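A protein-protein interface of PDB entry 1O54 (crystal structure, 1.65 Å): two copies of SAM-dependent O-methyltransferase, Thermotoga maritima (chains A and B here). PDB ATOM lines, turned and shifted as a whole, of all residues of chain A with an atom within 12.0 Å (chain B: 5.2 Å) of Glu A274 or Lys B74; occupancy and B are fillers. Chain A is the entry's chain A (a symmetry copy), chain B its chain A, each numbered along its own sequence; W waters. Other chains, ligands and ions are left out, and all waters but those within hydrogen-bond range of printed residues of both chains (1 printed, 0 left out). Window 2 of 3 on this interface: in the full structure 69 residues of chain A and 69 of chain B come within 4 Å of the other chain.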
ATOM      1  N   TRP A 200      24.501 -12.249 -25.360  1.00  0.00           N
ATOM      2  CA  TRP A 200      24.302 -13.291 -24.359  1.00  0.00           C
ATOM      3  C   TRP A 200      23.682 -12.707 -23.090  1.00  0.00           C
ATOM      4  O   TRP A 200      22.732 -13.262 -22.544  1.00  0.00           O
ATOM      5  CB  TRP A 200      25.631 -14.007 -24.055  1.00  0.00           C
ATOM      6  CG  TRP A 200      25.491 -15.193 -23.131  1.00  0.00           C
ATOM      7  CD1 TRP A 200      25.302 -16.500 -23.476  1.00  0.00           C
ATOM      8  CD2 TRP A 200      25.490 -15.156 -21.706  1.00  0.00           C
ATOM      9  NE1 TRP A 200      25.187 -17.281 -22.352  1.00  0.00           N
ATOM     10  CE2 TRP A 200      25.283 -16.484 -21.249  1.00  0.00           C
ATOM     11  CE3 TRP A 200      25.646 -14.134 -20.756  1.00  0.00           C
ATOM     12  CZ2 TRP A 200      25.260 -16.815 -19.890  1.00  0.00           C
ATOM     13  CZ3 TRP A 200      25.561 -14.458 -19.414  1.00  0.00           C
ATOM     14  CH2 TRP A 200      25.375 -15.800 -18.995  1.00  0.00           C
ATOM     15  N   LEU A 226      31.060 -17.358 -30.318  1.00  0.00           N
ATOM     16  CA  LEU A 226      29.941 -18.099 -29.739  1.00  0.00           C
ATOM     17  C   LEU A 226      30.413 -19.269 -28.861  1.00  0.00           C
ATOM     18  O   LEU A 226      29.847 -19.538 -27.786  1.00  0.00           O
ATOM     19  CB  LEU A 226      28.993 -18.627 -30.845  1.00  0.00           C
ATOM     20  CG  LEU A 226      28.133 -17.563 -31.528  1.00  0.00           C
ATOM     21  CD1 LEU A 226      27.487 -18.139 -32.754  1.00  0.00           C
ATOM     22  CD2 LEU A 226      27.026 -17.016 -30.622  1.00  0.00           C
ATOM     23  N   GLN A 227      31.446 -19.955 -29.331  1.00  0.00           N
ATOM     24  CA  GLN A 227      31.946 -21.137 -28.664  1.00  0.00           C
ATOM     25  C   GLN A 227      32.688 -20.793 -27.382  1.00  0.00           C
ATOM     26  O   GLN A 227      32.912 -21.665 -26.555  1.00  0.00           O
ATOM     27  CB  GLN A 227      32.736 -22.022 -29.649  1.00  0.00           C
ATOM     28  CG  GLN A 227      31.692 -22.668 -30.589  1.00  0.00           C
ATOM     29  CD  GLN A 227      32.227 -23.438 -31.757  1.00  0.00           C
ATOM     30  OE1 GLN A 227      33.432 -23.526 -31.939  1.00  0.00           O
ATOM     31  NE2 GLN A 227      31.301 -24.001 -32.570  1.00  0.00           N
ATOM     32  N   GLU A 228      33.045 -19.532 -27.192  1.00  0.00           N
ATOM     33  CA  GLU A 228      33.664 -19.093 -25.943  1.00  0.00           C
ATOM     34  C   GLU A 228      32.630 -18.859 -24.832  1.00  0.00           C
ATOM     35  O   GLU A 228      33.010 -18.776 -23.669  1.00  0.00           O
ATOM     36  CB  GLU A 228      34.466 -17.817 -26.177  1.00  0.00           C
ATOM     37  CG  GLU A 228      35.683 -18.082 -27.048  1.00  0.00           C
ATOM     38  CD  GLU A 228      36.383 -16.824 -27.538  1.00  0.00           C
ATOM     39  OE1 GLU A 228      35.997 -15.697 -27.152  1.00  0.00           O
ATOM     40  OE2 GLU A 228      37.353 -16.991 -28.318  1.00  0.00           O
ATOM     41  N   LEU A 229      31.349 -18.732 -25.197  1.00  0.00           N
ATOM     42  CA  LEU A 229      30.273 -18.349 -24.272  1.00  0.00           C
ATOM     43  C   LEU A 229      29.274 -19.498 -24.065  1.00  0.00           C
ATOM     44  O   LEU A 229      29.328 -20.505 -24.791  1.00  0.00           O
ATOM     45  CB  LEU A 229      29.542 -17.130 -24.819  1.00  0.00           C
ATOM     46  CG  LEU A 229      30.238 -15.778 -24.695  1.00  0.00           C
ATOM     47  CD1 LEU A 229      29.569 -14.828 -25.626  1.00  0.00           C
ATOM     48  CD2 LEU A 229      30.140 -15.289 -23.289  1.00  0.00           C
ATOM     49  N   PRO A 230      28.399 -19.403 -23.052  1.00  0.00           N
ATOM     50  CA  PRO A 230      27.398 -20.446 -22.821  1.00  0.00           C
ATOM     51  C   PRO A 230      26.227 -20.410 -23.840  1.00  0.00           C
ATOM     52  O   PRO A 230      25.132 -19.904 -23.561  1.00  0.00           O
ATOM     53  CB  PRO A 230      26.952 -20.192 -21.375  1.00  0.00           C
ATOM     54  CG  PRO A 230      27.972 -19.301 -20.800  1.00  0.00           C
ATOM     55  CD  PRO A 230      28.367 -18.419 -21.962  1.00  0.00           C
ATOM     56  N   PHE A 231      26.519 -21.017 -24.979  1.00  0.00           N
ATOM     57  CA  PHE A 231      25.591 -21.175 -26.103  1.00  0.00           C
ATOM     58  C   PHE A 231      25.639 -22.632 -26.536  1.00  0.00           C
ATOM     59  O   PHE A 231      26.744 -23.258 -26.584  1.00  0.00           O
ATOM     60  CB  PHE A 231      26.032 -20.324 -27.272  1.00  0.00           C
ATOM     61  CG  PHE A 231      25.622 -18.863 -27.192  1.00  0.00           C
ATOM     62  CD1 PHE A 231      26.589 -17.855 -27.063  1.00  0.00           C
ATOM     63  CD2 PHE A 231      24.288 -18.501 -27.262  1.00  0.00           C
ATOM     64  CE1 PHE A 231      26.210 -16.522 -27.025  1.00  0.00           C
ATOM     65  CE2 PHE A 231      23.917 -17.169 -27.228  1.00  0.00           C
ATOM     66  CZ  PHE A 231      24.879 -16.183 -27.131  1.00  0.00           C
ATOM     67  N   ILE A 232      24.468 -23.186 -26.846  1.00  0.00           N
ATOM     68  CA  ILE A 232      24.362 -24.544 -27.378  1.00  0.00           C
ATOM     69  C   ILE A 232      23.528 -24.505 -28.644  1.00  0.00           C
ATOM     70  O   ILE A 232      23.009 -23.424 -29.031  1.00  0.00           O
ATOM     71  CB  ILE A 232      23.774 -25.515 -26.311  1.00  0.00           C
ATOM     72  CG1 ILE A 232      22.331 -25.116 -25.985  1.00  0.00           C
ATOM     73  CG2 ILE A 232      24.677 -25.531 -25.058  1.00  0.00           C
ATOM     74  CD1 ILE A 232      21.588 -26.207 -25.233  1.00  0.00           C
ATOM     75  N   ARG A 233      23.361 -25.689 -29.283  1.00  0.00           N
ATOM     76  CA  ARG A 233      22.539 -25.809 -30.499  1.00  0.00           C
ATOM     77  C   ARG A 233      22.996 -24.758 -31.525  1.00  0.00           C
ATOM     78  O   ARG A 233      22.187 -24.088 -32.173  1.00  0.00           O
ATOM     79  CB  ARG A 233      21.042 -25.689 -30.176  1.00  0.00           C
ATOM     80  CG  ARG A 233      20.518 -26.771 -29.231  1.00  0.00           C
ATOM     81  CD  ARG A 233      19.014 -26.643 -28.982  1.00  0.00           C
ATOM     82  NE  ARG A 233      18.242 -27.347 -29.993  1.00  0.00           N
ATOM     83  CZ  ARG A 233      16.932 -27.258 -30.157  1.00  0.00           C
ATOM     84  NH1 ARG A 233      16.196 -26.482 -29.388  1.00  0.00           N
ATOM     85  NH2 ARG A 233      16.350 -27.964 -31.092  1.00  0.00           N
ATOM     86  N   ILE A 234      24.306 -24.653 -31.713  1.00  0.00           N
ATOM     87  CA  ILE A 234      24.834 -23.687 -32.701  1.00  0.00           C
ATOM     88  C   ILE A 234      24.698 -24.317 -34.072  1.00  0.00           C
ATOM     89  O   ILE A 234      25.173 -25.465 -34.319  1.00  0.00           O
ATOM     90  CB  ILE A 234      26.318 -23.323 -32.405  1.00  0.00           C
ATOM     91  CG1 ILE A 234      26.428 -22.628 -31.061  1.00  0.00           C
ATOM     92  CG2 ILE A 234      26.866 -22.390 -33.495  1.00  0.00           C
ATOM     93  CD1 ILE A 234      27.799 -22.569 -30.520  1.00  0.00           C
ATOM     94  N   THR A 268      21.490 -20.976 -28.994  1.00  0.00           N
ATOM     95  CA  THR A 268      20.580 -20.892 -27.858  1.00  0.00           C
ATOM     96  C   THR A 268      21.369 -20.618 -26.600  1.00  0.00           C
ATOM     97  O   THR A 268      22.310 -21.352 -26.322  1.00  0.00           O
ATOM     98  CB  THR A 268      19.837 -22.229 -27.748  1.00  0.00           C
ATOM     99  OG1 THR A 268      19.006 -22.412 -28.918  1.00  0.00           O
ATOM    100  CG2 THR A 268      18.908 -22.242 -26.543  1.00  0.00           C
ATOM    101  N   LYS A 269      20.971 -19.594 -25.855  1.00  0.00           N
ATOM    102  CA  LYS A 269      21.612 -19.244 -24.603  1.00  0.00           C
ATOM    103  C   LYS A 269      21.287 -20.225 -23.504  1.00  0.00           C
ATOM    104  O   LYS A 269      20.119 -20.560 -23.264  1.00  0.00           O
ATOM    105  CB  LYS A 269      21.178 -17.852 -24.157  1.00  0.00           C
ATOM    106  CG  LYS A 269      21.907 -17.338 -22.875  1.00  0.00           C
ATOM    107  CD  LYS A 269      21.032 -16.654 -22.004  1.00  0.00           C
ATOM    108  CE  LYS A 269      21.587 -16.349 -20.639  1.00  0.00           C
ATOM    109  NZ  LYS A 269      21.719 -14.893 -20.477  1.00  0.00           N
ATOM    110  N   VAL A 270      22.322 -20.638 -22.789  1.00  0.00           N
ATOM    111  CA  VAL A 270      22.161 -21.349 -21.525  1.00  0.00           C
ATOM    112  C   VAL A 270      22.860 -20.559 -20.424  1.00  0.00           C
ATOM    113  O   VAL A 270      23.651 -19.649 -20.701  1.00  0.00           O
ATOM    114  CB  VAL A 270      22.669 -22.771 -21.619  1.00  0.00           C
ATOM    115  CG1 VAL A 270      21.800 -23.548 -22.615  1.00  0.00           C
ATOM    116  CG2 VAL A 270      24.176 -22.826 -21.999  1.00  0.00           C
ATOM    117  N   CYS A 271      22.560 -20.884 -19.177  1.00  0.00           N
ATOM    118  CA  CYS A 271      23.059 -20.081 -18.061  1.00  0.00           C
ATOM    119  C   CYS A 271      24.552 -20.271 -17.820  1.00  0.00           C
ATOM    120  O   CYS A 271      25.244 -19.324 -17.467  1.00  0.00           O
ATOM    121  CB  CYS A 271      22.268 -20.380 -16.787  1.00  0.00           C
ATOM    122  SG  CYS A 271      20.548 -19.858 -17.015  1.00  0.00           S
ATOM    123  N   ARG A 272      25.047 -21.481 -18.026  1.00  0.00           N
ATOM    124  CA  ARG A 272      26.457 -21.746 -17.749  1.00  0.00           C
ATOM    125  C   ARG A 272      26.901 -23.020 -18.423  1.00  0.00           C
ATOM    126  O   ARG A 272      26.091 -23.855 -18.811  1.00  0.00           O
ATOM    127  CB  ARG A 272      26.729 -21.787 -16.236  1.00  0.00           C
ATOM    128  CG  ARG A 272      25.701 -22.552 -15.437  1.00  0.00           C
ATOM    129  CD  ARG A 272      25.917 -22.545 -13.924  1.00  0.00           C
ATOM    130  NE  ARG A 272      25.254 -23.701 -13.328  1.00  0.00           N
ATOM    131  CZ  ARG A 272      25.257 -24.003 -12.024  1.00  0.00           C
ATOM    132  NH1 ARG A 272      25.899 -23.243 -11.139  1.00  0.00           N
ATOM    133  NH2 ARG A 272      24.617 -25.094 -11.610  1.00  0.00           N
ATOM    134  N   ARG A 273      28.212 -23.148 -18.545  1.00  0.00           N
ATOM    135  CA  ARG A 273      28.826 -24.260 -19.255  1.00  0.00           C
ATOM    136  C   ARG A 273      28.889 -25.470 -18.322  1.00  0.00           C
ATOM    137  O   ARG A 273      28.721 -26.607 -18.755  1.00  0.00           O
ATOM    138  CB  ARG A 273      30.239 -23.880 -19.739  1.00  0.00           C
ATOM    139  CG  ARG A 273      30.440 -22.373 -20.026  1.00  0.00           C
ATOM    140  CD  ARG A 273      31.023 -22.025 -21.381  1.00  0.00           C
ATOM    141  NE  ARG A 273      32.010 -23.001 -21.851  1.00  0.00           N
ATOM    142  CZ  ARG A 273      32.258 -23.274 -23.136  1.00  0.00           C
ATOM    143  NH1 ARG A 273      31.589 -22.655 -24.114  1.00  0.00           N
ATOM    144  NH2 ARG A 273      33.176 -24.190 -23.446  1.00  0.00           N
ATOM    145  N   GLU A 274      29.103 -25.200 -17.038  1.00  0.00           N
ATOM    146  CA  GLU A 274      29.255 -26.242 -16.021  1.00  0.00           C
ATOM    147  C   GLU A 274      28.659 -25.746 -14.717  1.00  0.00           C
ATOM    148  O   GLU A 274      28.529 -24.529 -14.505  1.00  0.00           O
ATOM    149  CB  GLU A 274      30.744 -26.567 -15.792  1.00  0.00           C
ATOM    150  CG  GLU A 274      31.475 -27.149 -16.994  1.00  0.00           C
ATOM    151  CD  GLU A 274      30.950 -28.519 -17.401  1.00  0.00           C
ATOM    152  OE1 GLU A 274      30.425 -29.246 -16.521  1.00  0.00           O
ATOM    153  OE2 GLU A 274      31.058 -28.869 -18.602  1.00  0.00           O
ATOM    154  N   GLU A 275      28.303 -26.677 -13.835  1.00  0.00           N
ATOM    155  CA  GLU A 275      27.833 -26.294 -12.508  1.00  0.00           C
ATOM    156  C   GLU A 275      28.988 -25.661 -11.731  1.00  0.00           C
ATOM    157  O   GLU A 275      30.153 -25.981 -11.962  1.00  0.00           O
ATOM    158  CB  GLU A 275      27.277 -27.488 -11.722  1.00  0.00           C
ATOM    159  CG  GLU A 275      25.966 -28.058 -12.250  1.00  0.00           C
ATOM    160  CD  GLU A 275      26.146 -29.329 -13.055  1.00  0.00           C
ATOM    161  OE1 GLU A 275      27.109 -29.398 -13.849  1.00  0.00           O
ATOM    162  OE2 GLU A 275      25.312 -30.255 -12.904  1.00  0.00           O
ATOM    163  N   SER B  29      18.244 -31.118 -24.066  1.00  0.00           N
ATOM    164  CA  SER B  29      19.238 -31.133 -25.137  1.00  0.00           C
ATOM    165  C   SER B  29      20.612 -31.522 -24.590  1.00  0.00           C
ATOM    166  O   SER B  29      21.101 -30.901 -23.656  1.00  0.00           O
ATOM    167  CB  SER B  29      19.275 -29.754 -25.783  1.00  0.00           C
ATOM    168  OG  SER B  29      20.189 -29.722 -26.855  1.00  0.00           O
ATOM    169  N   PHE B  30      21.246 -32.543 -25.183  1.00  0.00           N
ATOM    170  CA  PHE B  30      22.499 -33.101 -24.669  1.00  0.00           C
ATOM    171  C   PHE B  30      23.733 -32.833 -25.555  1.00  0.00           C
ATOM    172  O   PHE B  30      23.594 -32.480 -26.716  1.00  0.00           O
ATOM    173  CB  PHE B  30      22.280 -34.595 -24.392  1.00  0.00           C
ATOM    174  CG  PHE B  30      21.388 -34.828 -23.206  1.00  0.00           C
ATOM    175  CD1 PHE B  30      20.010 -34.855 -23.357  1.00  0.00           C
ATOM    176  CD2 PHE B  30      21.923 -34.943 -21.932  1.00  0.00           C
ATOM    177  CE1 PHE B  30      19.183 -35.001 -22.254  1.00  0.00           C
ATOM    178  CE2 PHE B  30      21.103 -35.081 -20.835  1.00  0.00           C
ATOM    179  CZ  PHE B  30      19.725 -35.113 -21.010  1.00  0.00           C
ATOM    180  N   GLU B  31      24.930 -33.011 -24.976  1.00  0.00           N
ATOM    181  CA  GLU B  31      26.216 -32.745 -25.663  1.00  0.00           C
ATOM    182  C   GLU B  31      26.362 -33.456 -27.016  1.00  0.00           C
ATOM    183  O   GLU B  31      26.908 -32.874 -27.963  1.00  0.00           O
ATOM    184  CB  GLU B  31      27.419 -33.111 -24.775  1.00  0.00           C
ATOM    185  CG  GLU B  31      27.588 -32.285 -23.493  1.00  0.00           C
ATOM    186  CD  GLU B  31      28.753 -32.756 -22.620  1.00  0.00           C
ATOM    187  OE1 GLU B  31      29.053 -33.981 -22.601  1.00  0.00           O
ATOM    188  OE2 GLU B  31      29.374 -31.909 -21.931  1.00  0.00           O
ATOM    189  N   ILE B  66      21.079 -26.636 -16.373  1.00  0.00           N
ATOM    190  CA  ILE B  66      21.601 -27.985 -16.544  1.00  0.00           C
ATOM    191  C   ILE B  66      20.747 -29.033 -15.834  1.00  0.00           C
ATOM    192  O   ILE B  66      20.265 -28.835 -14.700  1.00  0.00           O
ATOM    193  CB  ILE B  66      23.055 -28.037 -16.008  1.00  0.00           C
ATOM    194  CG1 ILE B  66      23.961 -27.252 -16.962  1.00  0.00           C
ATOM    195  CG2 ILE B  66      23.524 -29.472 -15.826  1.00  0.00           C
ATOM    196  CD1 ILE B  66      25.332 -26.916 -16.423  1.00  0.00           C
ATOM    197  N   ILE B  67      20.623 -30.175 -16.495  1.00  0.00           N
ATOM    198  CA  ILE B  67      20.070 -31.381 -15.904  1.00  0.00           C
ATOM    199  C   ILE B  67      21.056 -32.507 -16.237  1.00  0.00           C
ATOM    200  O   ILE B  67      21.550 -32.589 -17.357  1.00  0.00           O
ATOM    201  CB  ILE B  67      18.627 -31.652 -16.443  1.00  0.00           C
ATOM    202  CG1 ILE B  67      17.994 -32.895 -15.804  1.00  0.00           C
ATOM    203  CG2 ILE B  67      18.613 -31.824 -17.941  1.00  0.00           C
ATOM    204  CD1 ILE B  67      17.616 -32.727 -14.378  1.00  0.00           C
ATOM    205  N   ARG B  68      21.359 -33.339 -15.241  1.00  0.00           N
ATOM    206  CA  ARG B  68      22.249 -34.484 -15.406  1.00  0.00           C
ATOM    207  C   ARG B  68      21.447 -35.784 -15.408  1.00  0.00           C
ATOM    208  O   ARG B  68      20.469 -35.935 -14.664  1.00  0.00           O
ATOM    209  CB  ARG B  68      23.242 -34.558 -14.248  1.00  0.00           C
ATOM    210  CG  ARG B  68      24.222 -33.398 -14.171  1.00  0.00           C
ATOM    211  CD  ARG B  68      25.586 -33.724 -14.733  1.00  0.00           C
ATOM    212  NE  ARG B  68      26.454 -32.551 -14.773  1.00  0.00           N
ATOM    213  CZ  ARG B  68      27.568 -32.476 -15.493  1.00  0.00           C
ATOM    214  NH1 ARG B  68      27.985 -33.515 -16.215  1.00  0.00           N
ATOM    215  NH2 ARG B  68      28.278 -31.354 -15.490  1.00  0.00           N
ATOM    216  N   GLY B  72      25.601 -39.225 -15.332  1.00  0.00           N
ATOM    217  CA  GLY B  72      26.416 -38.012 -15.226  1.00  0.00           C
ATOM    218  C   GLY B  72      26.488 -37.157 -16.478  1.00  0.00           C
ATOM    219  O   GLY B  72      27.189 -36.151 -16.485  1.00  0.00           O
ATOM    220  N   LYS B  73      25.773 -37.553 -17.531  1.00  0.00           N
ATOM    221  CA  LYS B  73      25.790 -36.836 -18.803  1.00  0.00           C
ATOM    222  C   LYS B  73      25.055 -35.500 -18.640  1.00  0.00           C
ATOM    223  O   LYS B  73      24.015 -35.439 -18.005  1.00  0.00           O
ATOM    224  CB  LYS B  73      25.111 -37.663 -19.894  1.00  0.00           C
ATOM    225  CG  LYS B  73      25.786 -39.014 -20.192  1.00  0.00           C
ATOM    226  CD  LYS B  73      26.871 -38.876 -21.253  1.00  0.00           C
ATOM    227  N   LYS B  74      25.607 -34.445 -19.224  1.00  0.00           N
ATOM    228  CA  LYS B  74      25.092 -33.087 -19.046  1.00  0.00           C
ATOM    229  C   LYS B  74      24.123 -32.723 -20.172  1.00  0.00           C
ATOM    230  O   LYS B  74      24.480 -32.765 -21.364  1.00  0.00           O
ATOM    231  CB  LYS B  74      26.260 -32.078 -19.032  1.00  0.00           C
ATOM    232  CG  LYS B  74      25.857 -30.631 -18.692  1.00  0.00           C
ATOM    233  CD  LYS B  74      27.041 -29.651 -18.799  1.00  0.00           C
ATOM    234  CE  LYS B  74      27.394 -29.370 -20.250  1.00  0.00           C
ATOM    235  NZ  LYS B  74      28.503 -28.406 -20.402  1.00  0.00           N
ATOM    236  N   GLY B  75      22.908 -32.340 -19.796  1.00  0.00           N
ATOM    237  CA  GLY B  75      21.958 -31.778 -20.746  1.00  0.00           C
ATOM    238  C   GLY B  75      21.444 -30.440 -20.273  1.00  0.00           C
ATOM    239  O   GLY B  75      21.729 -30.017 -19.161  1.00  0.00           O
ATOM    240  N   TYR B  76      20.675 -29.784 -21.127  1.00  0.00           N
ATOM    241  CA  TYR B  76      20.072 -28.496 -20.813  1.00  0.00           C
ATOM    242  C   TYR B  76      18.562 -28.533 -21.013  1.00  0.00           C
ATOM    243  O   TYR B  76      18.064 -29.132 -21.963  1.00  0.00           O
ATOM    244  CB  TYR B  76      20.684 -27.439 -21.726  1.00  0.00           C
ATOM    245  CG  TYR B  76      22.097 -27.132 -21.359  1.00  0.00           C
ATOM    246  CD1 TYR B  76      23.154 -27.762 -22.004  1.00  0.00           C
ATOM    247  CD2 TYR B  76      22.384 -26.198 -20.373  1.00  0.00           C
ATOM    248  CE1 TYR B  76      24.467 -27.453 -21.671  1.00  0.00           C
ATOM    249  CE2 TYR B  76      23.685 -25.895 -20.024  1.00  0.00           C
ATOM    250  CZ  TYR B  76      24.724 -26.531 -20.678  1.00  0.00           C
ATOM    251  OH  TYR B  76      26.019 -26.212 -20.333  1.00  0.00           O
HETATM  252  O   HOH W   1      22.572 -24.409 -14.460  1.00  0.00           O
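The guanidinium group of Arg B68 lies within salt-bridge range of the side-chain carboxylate of Glu A274 (3.2 Å).
NH2 of Arg B68 is in salt-bridge range of OE1 of Glu A275 (2.8 Å).
The side-chain amino group (NZ) of Lys B74 sits at hydrogen-bond distance from the backbone carbonyl oxygen (O) of Arg A273 (2.4 Å).
The side-chain amino group (NZ) of Lys B74 lies within salt-bridge range of the side-chain carboxylate (OE2) of Glu A274, 3.2 Å away.
O of Arg A272 is in hydrogen-bond range of OH of Tyr B76, 2.8 Å away.
The side-chain hydroxyl (OH) of Tyr B76 lies within hydrogen-bond range of the backbone carbonyl oxygen (O) of Arg A273 (3.2 Å).
O of Ser B29 sits at hydrogen-bond distance from N of Tyr B76 (2.8 Å).
NZ of Lys B74 is in salt-bridge range of OE2 of Glu B31, 3.9 Å away.
The side-chain hydroxyl of Tyr B76 sits at hydrogen-bond distance from the side-chain amino group of Lys B74 (3.3 Å).
The guanidinium group (NH1) of Arg A273 is in hydrogen-bond range of the backbone carbonyl oxygen (O) of Gln A227.
The backbone carbonyl oxygen (O) of Pro A230 lies within hydrogen-bond range of the backbone NH (N) of Val A270 (3.0 Å).
O of Thr A268 is in hydrogen-bond range of N of Ile A232 (2.9 Å).
Ile A232 touches Tyr B76.
CG of Arg A233 touches OG of Ser B29, at 3.8 Å.
Val A270 touches Tyr B76 (CG1 to CD2, 3.5 Å).
O of Arg A272 touches CD1 of Ile B66, 3.96 Å away.
Glu A274 touches Ile B66 (C to CD1, 3.9 Å).
Glu A275 touches Ile B66.
Of the printed residues of chain B, Ile A232 touches Tyr B76 (3.8 Å).
Printed residues of chain B within 4 Å of Arg A272: Ile B66 and Tyr B76.
Printed residues of chain B within 4 Å of Arg A273: Lys B74 and Tyr B76.
Of chain B, only Ile B66 (3.9 Å), Arg B68 (3.2 Å) and Lys B74 (3.2 Å) come within 4 Å of Glu A274.
Of the printed residues of chain B, Glu A275 touches Ile B66 (3.5 Å) and Arg B68 (2.8 Å).
Of chain A, only Arg A233 (3.8 Å) comes within 4 Å of Ser B29.
No residue of chain A comes within 4 Å of Glu B31.
Of the printed residues of chain A, Ile B66 touches Arg A272, Glu A274 and Glu A275.
No residue of chain A comes within 4 Å of Gly B72.
Lys B73 touches none of the printed residues of chain A.
The nearest residue of chain A that does not touch Lys B74 is Glu A275 (5.0 Å).
The nearest printed residue of chain B that does not touch Arg A233 is Phe B30 (7.0 Å).
Of the 18 printed residues of chain A, 7 touch a printed residue of chain B.
Hydrophobic or aromatic side chains of chain A that line the printed part of chain B: Ile A232 and Val A270.
Along chain A the printed residues that touch a printed residue of chain B span positions 232 to 275.
Among the printed residues, 12 pairs touch across the chains.
No position is printed for both chains.
Water W1 lies within hydrogen-bond range of the guanidinium group of Arg A272 (3.0 Å) and the backbone NH of Ile B66 (3.3 Å).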
